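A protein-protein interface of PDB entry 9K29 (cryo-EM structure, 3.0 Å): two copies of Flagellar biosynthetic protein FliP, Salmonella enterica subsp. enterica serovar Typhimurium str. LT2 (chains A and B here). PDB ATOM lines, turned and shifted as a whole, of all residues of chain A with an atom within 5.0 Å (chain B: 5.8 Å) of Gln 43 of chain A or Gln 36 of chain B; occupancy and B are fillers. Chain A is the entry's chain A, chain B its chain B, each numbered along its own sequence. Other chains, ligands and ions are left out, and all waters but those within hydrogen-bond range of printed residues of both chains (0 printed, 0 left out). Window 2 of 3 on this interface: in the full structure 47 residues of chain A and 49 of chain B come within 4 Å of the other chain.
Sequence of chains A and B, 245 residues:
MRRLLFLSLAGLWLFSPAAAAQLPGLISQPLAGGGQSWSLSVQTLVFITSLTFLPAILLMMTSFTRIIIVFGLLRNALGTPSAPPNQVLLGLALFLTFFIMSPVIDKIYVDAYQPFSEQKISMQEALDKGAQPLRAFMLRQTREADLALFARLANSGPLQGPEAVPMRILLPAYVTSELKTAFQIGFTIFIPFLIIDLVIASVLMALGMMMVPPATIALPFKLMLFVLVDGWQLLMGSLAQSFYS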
ATOM      1  N   SER A  39     -29.457 -22.675  16.663  1.00  0.00           N
ATOM      2  CA  SER A  39     -29.018 -21.320  16.349  1.00  0.00           C
ATOM      3  C   SER A  39     -28.468 -20.602  17.574  1.00  0.00           C
ATOM      4  O   SER A  39     -27.839 -19.545  17.438  1.00  0.00           O
ATOM      5  CB  SER A  39     -30.174 -20.519  15.748  1.00  0.00           C
ATOM      6  OG  SER A  39     -31.217 -20.343  16.690  1.00  0.00           O
ATOM      7  N   LEU A  40     -28.700 -21.148  18.770  1.00  0.00           N
ATOM      8  CA  LEU A  40     -28.171 -20.538  19.984  1.00  0.00           C
ATOM      9  C   LEU A  40     -26.648 -20.574  19.998  1.00  0.00           C
ATOM     10  O   LEU A  40     -25.997 -19.662  20.523  1.00  0.00           O
ATOM     11  CB  LEU A  40     -28.739 -21.252  21.211  1.00  0.00           C
ATOM     12  CG  LEU A  40     -30.256 -21.155  21.392  1.00  0.00           C
ATOM     13  CD1 LEU A  40     -30.711 -21.993  22.577  1.00  0.00           C
ATOM     14  CD2 LEU A  40     -30.699 -19.709  21.548  1.00  0.00           C
ATOM     15  N   SER A  41     -26.061 -21.621  19.419  1.00  0.00           N
ATOM     16  CA  SER A  41     -24.611 -21.726  19.324  1.00  0.00           C
ATOM     17  C   SER A  41     -24.007 -20.728  18.348  1.00  0.00           C
ATOM     18  O   SER A  41     -22.796 -20.489  18.399  1.00  0.00           O
ATOM     19  CB  SER A  41     -24.209 -23.144  18.913  1.00  0.00           C
ATOM     20  OG  SER A  41     -22.799 -23.260  18.845  1.00  0.00           O
ATOM     21  N   VAL A  42     -24.812 -20.154  17.452  1.00  0.00           N
ATOM     22  CA  VAL A  42     -24.328 -19.061  16.617  1.00  0.00           C
ATOM     23  C   VAL A  42     -24.623 -17.725  17.284  1.00  0.00           C
ATOM     24  O   VAL A  42     -23.874 -16.751  17.128  1.00  0.00           O
ATOM     25  CB  VAL A  42     -24.950 -19.150  15.211  1.00  0.00           C
ATOM     26  CG1 VAL A  42     -24.382 -18.071  14.302  1.00  0.00           C
ATOM     27  CG2 VAL A  42     -24.722 -20.530  14.619  1.00  0.00           C
ATOM     28  N   GLN A  43     -25.715 -17.662  18.048  1.00  0.00           N
ATOM     29  CA  GLN A  43     -26.036 -16.457  18.804  1.00  0.00           C
ATOM     30  C   GLN A  43     -24.953 -16.160  19.833  1.00  0.00           C
ATOM     31  O   GLN A  43     -24.586 -15.004  20.057  1.00  0.00           O
ATOM     32  CB  GLN A  43     -27.400 -16.608  19.479  1.00  0.00           C
ATOM     33  CG  GLN A  43     -27.888 -15.347  20.171  1.00  0.00           C
ATOM     34  CD  GLN A  43     -29.277 -15.503  20.754  1.00  0.00           C
ATOM     35  OE1 GLN A  43     -29.874 -16.577  20.686  1.00  0.00           O
ATOM     36  NE2 GLN A  43     -29.800 -14.428  21.332  1.00  0.00           N
ATOM     37  N   THR A  44     -24.425 -17.206  20.475  1.00  0.00           N
ATOM     38  CA  THR A  44     -23.354 -16.998  21.447  1.00  0.00           C
ATOM     39  C   THR A  44     -22.070 -16.523  20.767  1.00  0.00           C
ATOM     40  O   THR A  44     -21.330 -15.706  21.328  1.00  0.00           O
ATOM     41  CB  THR A  44     -23.109 -18.273  22.259  1.00  0.00           C
ATOM     42  OG1 THR A  44     -22.132 -18.015  23.274  1.00  0.00           O
ATOM     43  CG2 THR A  44     -22.632 -19.411  21.378  1.00  0.00           C
ATOM     44  N   LEU A  45     -21.795 -17.011  19.555  1.00  0.00           N
ATOM     45  CA  LEU A  45     -20.626 -16.532  18.820  1.00  0.00           C
ATOM     46  C   LEU A  45     -20.785 -15.067  18.435  1.00  0.00           C
ATOM     47  O   LEU A  45     -19.835 -14.280  18.537  1.00  0.00           O
ATOM     48  CB  LEU A  45     -20.395 -17.395  17.581  1.00  0.00           C
ATOM     49  CG  LEU A  45     -19.991 -18.847  17.841  1.00  0.00           C
ATOM     50  CD1 LEU A  45     -19.916 -19.628  16.539  1.00  0.00           C
ATOM     51  CD2 LEU A  45     -18.669 -18.910  18.586  1.00  0.00           C
ATOM     52  N   VAL A  46     -21.984 -14.683  17.988  1.00  0.00           N
ATOM     53  CA  VAL A  46     -22.262 -13.277  17.723  1.00  0.00           C
ATOM     54  C   VAL A  46     -22.135 -12.443  18.992  1.00  0.00           C
ATOM     55  O   VAL A  46     -21.645 -11.309  18.942  1.00  0.00           O
ATOM     56  CB  VAL A  46     -23.658 -13.115  17.093  1.00  0.00           C
ATOM     57  CG1 VAL A  46     -24.012 -11.645  16.932  1.00  0.00           C
ATOM     58  CG2 VAL A  46     -23.715 -13.824  15.751  1.00  0.00           C
ATOM     59  N   PHE A  47     -22.558 -12.987  20.134  1.00  0.00           N
ATOM     60  CA  PHE A  47     -22.410 -12.284  21.404  1.00  0.00           C
ATOM     61  C   PHE A  47     -20.940 -12.063  21.738  1.00  0.00           C
ATOM     62  O   PHE A  47     -20.556 -10.991  22.212  1.00  0.00           O
ATOM     63  CB  PHE A  47     -23.108 -13.066  22.516  1.00  0.00           C
ATOM     64  CG  PHE A  47     -22.809 -12.557  23.897  1.00  0.00           C
ATOM     65  CD1 PHE A  47     -23.400 -11.396  24.365  1.00  0.00           C
ATOM     66  CD2 PHE A  47     -21.944 -13.245  24.731  1.00  0.00           C
ATOM     67  CE1 PHE A  47     -23.128 -10.927  25.635  1.00  0.00           C
ATOM     68  CE2 PHE A  47     -21.668 -12.781  26.003  1.00  0.00           C
ATOM     69  CZ  PHE A  47     -22.261 -11.620  26.454  1.00  0.00           C
ATOM     70  N   SER B  28     -23.447 -21.333  28.775  1.00  0.00           N
ATOM     71  CA  SER B  28     -24.707 -20.838  28.223  1.00  0.00           C
ATOM     72  C   SER B  28     -25.787 -21.888  28.441  1.00  0.00           C
ATOM     73  O   SER B  28     -25.602 -23.055  28.085  1.00  0.00           O
ATOM     74  CB  SER B  28     -24.559 -20.509  26.740  1.00  0.00           C
ATOM     75  OG  SER B  28     -24.342 -21.682  25.976  1.00  0.00           O
ATOM     76  N   GLN B  29     -26.907 -21.473  29.024  1.00  0.00           N
ATOM     77  CA  GLN B  29     -28.065 -22.344  29.224  1.00  0.00           C
ATOM     78  C   GLN B  29     -29.322 -21.634  28.745  1.00  0.00           C
ATOM     79  O   GLN B  29     -29.560 -20.475  29.136  1.00  0.00           O
ATOM     80  CB  GLN B  29     -28.210 -22.742  30.695  1.00  0.00           C
ATOM     81  CG  GLN B  29     -26.986 -23.414  31.298  1.00  0.00           C
ATOM     82  CD  GLN B  29     -26.025 -22.426  31.930  1.00  0.00           C
ATOM     83  OE1 GLN B  29     -25.824 -21.324  31.422  1.00  0.00           O
ATOM     84  NE2 GLN B  29     -25.425 -22.819  33.047  1.00  0.00           N
ATOM     85  N   PRO B  30     -30.142 -22.259  27.904  1.00  0.00           N
ATOM     86  CA  PRO B  30     -31.377 -21.608  27.451  1.00  0.00           C
ATOM     87  C   PRO B  30     -32.358 -21.389  28.594  1.00  0.00           C
ATOM     88  O   PRO B  30     -32.399 -22.156  29.558  1.00  0.00           O
ATOM     89  CB  PRO B  30     -31.933 -22.589  26.413  1.00  0.00           C
ATOM     90  CG  PRO B  30     -30.764 -23.407  25.985  1.00  0.00           C
ATOM     91  CD  PRO B  30     -29.883 -23.518  27.187  1.00  0.00           C
ATOM     92  N   LEU B  31     -33.153 -20.329  28.478  1.00  0.00           N
ATOM     93  CA  LEU B  31     -34.215 -20.013  29.431  1.00  0.00           C
ATOM     94  C   LEU B  31     -35.535 -19.964  28.667  1.00  0.00           C
ATOM     95  O   LEU B  31     -35.785 -19.018  27.912  1.00  0.00           O
ATOM     96  CB  LEU B  31     -33.943 -18.695  30.153  1.00  0.00           C
ATOM     97  CG  LEU B  31     -33.108 -18.768  31.432  1.00  0.00           C
ATOM     98  CD1 LEU B  31     -31.642 -18.994  31.116  1.00  0.00           C
ATOM     99  CD2 LEU B  31     -33.291 -17.505  32.262  1.00  0.00           C
ATOM    100  N   GLY B  34     -36.862 -19.915  23.175  1.00  0.00           N
ATOM    101  CA  GLY B  34     -36.026 -18.985  22.439  1.00  0.00           C
ATOM    102  C   GLY B  34     -35.202 -18.061  23.312  1.00  0.00           C
ATOM    103  O   GLY B  34     -35.110 -16.860  23.041  1.00  0.00           O
ATOM    104  N   GLY B  35     -34.605 -18.619  24.370  1.00  0.00           N
ATOM    105  CA  GLY B  35     -33.796 -17.806  25.298  1.00  0.00           C
ATOM    106  C   GLY B  35     -32.403 -18.379  25.490  1.00  0.00           C
ATOM    107  O   GLY B  35     -32.212 -19.573  25.186  1.00  0.00           O
ATOM    108  N   GLN B  36     -31.463 -17.558  25.969  1.00  0.00           N
ATOM    109  CA  GLN B  36     -30.072 -18.024  26.216  1.00  0.00           C
ATOM    110  C   GLN B  36     -29.457 -17.170  27.330  1.00  0.00           C
ATOM    111  O   GLN B  36     -29.783 -15.971  27.394  1.00  0.00           O
ATOM    112  CB  GLN B  36     -29.250 -17.936  24.929  1.00  0.00           C
ATOM    113  CG  GLN B  36     -27.817 -18.428  25.081  1.00  0.00           C
ATOM    114  CD  GLN B  36     -27.075 -18.431  23.766  1.00  0.00           C
ATOM    115  OE1 GLN B  36     -25.919 -18.841  23.686  1.00  0.00           O
ATOM    116  NE2 GLN B  36     -27.740 -17.973  22.719  1.00  0.00           N
ATOM    117  N   SER B  37     -28.609 -17.767  28.171  1.00  0.00           N
ATOM    118  CA  SER B  37     -27.946 -17.014  29.267  1.00  0.00           C
ATOM    119  C   SER B  37     -26.430 -17.225  29.196  1.00  0.00           C
ATOM    120  O   SER B  37     -26.005 -18.392  29.137  1.00  0.00           O
ATOM    121  CB  SER B  37     -28.488 -17.427  30.609  1.00  0.00           C
ATOM    122  OG  SER B  37     -27.779 -16.781  31.658  1.00  0.00           O
ATOM    123  N   TRP B  38     -25.656 -16.137  29.209  1.00  0.00           N
ATOM    124  CA  TRP B  38     -24.176 -16.247  29.102  1.00  0.00           C
ATOM    125  C   TRP B  38     -23.530 -16.019  30.473  1.00  0.00           C
ATOM    126  O   TRP B  38     -23.360 -14.844  30.854  1.00  0.00           O
ATOM    127  CB  TRP B  38     -23.637 -15.269  28.050  1.00  0.00           C
ATOM    128  CG  TRP B  38     -24.068 -15.597  26.654  1.00  0.00           C
ATOM    129  CD1 TRP B  38     -23.559 -16.574  25.848  1.00  0.00           C
ATOM    130  CD2 TRP B  38     -25.101 -14.947  25.891  1.00  0.00           C
ATOM    131  NE1 TRP B  38     -24.203 -16.578  24.641  1.00  0.00           N
ATOM    132  CE2 TRP B  38     -25.153 -15.591  24.636  1.00  0.00           C
ATOM    133  CE3 TRP B  38     -25.981 -13.890  26.141  1.00  0.00           C
ATOM    134  CZ2 TRP B  38     -26.050 -15.210  23.641  1.00  0.00           C
ATOM    135  CZ3 TRP B  38     -26.868 -13.515  25.158  1.00  0.00           C
ATOM    136  CH2 TRP B  38     -26.902 -14.169  23.926  1.00  0.00           C
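The side-chain amide oxygen (OE1) of Gln 36 of chain B lies close to the backbone carbonyl oxygen (O) of Leu 40 of chain A (3.3 Å).
The side-chain amide oxygen of Gln 43 of chain A sits at hydrogen-bond distance from the side-chain amide nitrogen of Gln 36 of chain B (3.3 Å).
OG1 of Thr 44 of chain A sits at hydrogen-bond distance from NE1 of Trp 38 of chain B.
The side-chain amide oxygen (OE1) of Gln 36 of chain B lies within hydrogen-bond range of the indole nitrogen (NE1) of Trp 38 of chain B (3.0 Å).
Leu 40 of chain A touches Pro 30 of chain B (CD1 to CG, 3.7 Å).
Leu 40 of chain A touches Gly 35 of chain B (CD1 to O, 3.9 Å).
CZ2 of Trp 38 of chain B touches O of Gln 43 of chain A, at 3.9 Å.
Thr 44 of chain A touches Gln 36 of chain B.
Phe 47 of chain A touches Trp 38 of chain B (CD2 to CG, 3.7 Å).
Val 42 of chain A touches none of the printed residues of chain B.
Gln 43 of chain A touches two residues of chain B.
Val 46 of chain A touches none of the printed residues of chain B.
Of the printed residues of chain B, Phe 47 of chain A touches Trp 38 (3.7 Å).
Gln 36 of chain B touches just these residues of chain A: Leu 40, Gln 43 and Thr 44.
Of the printed residues of chain A, Trp 38 of chain B touches Gln 43, Thr 44 and Phe 47.
The nearest printed residue of chain B that does not touch Gln 43 of chain A is Gly 35 of chain B (5.7 Å).
The nearest printed residue of chain A that does not touch Gln 36 of chain B is Ser 41 of chain A (5.1 Å).
The nearest printed residue of chain A that does not touch Pro 30 of chain B is Ser 41 of chain A (8.3 Å).
Of the 9 printed residues of chain A, 4 touch a printed residue of chain B.
Of the 9 printed residues of chain B, 4 touch a printed residue of chain A.
Printed residues of chain B that touch a printed residue of chain A: Pro 30, Gly 35, Gln 36 and Trp 38.
Hydrophobic or aromatic side chains of chain B within 4 Å of the printed part of chain A: Pro 30 and Trp 38.
Among the printed residues, 8 pairs touch across the chains.
No position is printed for both chains.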
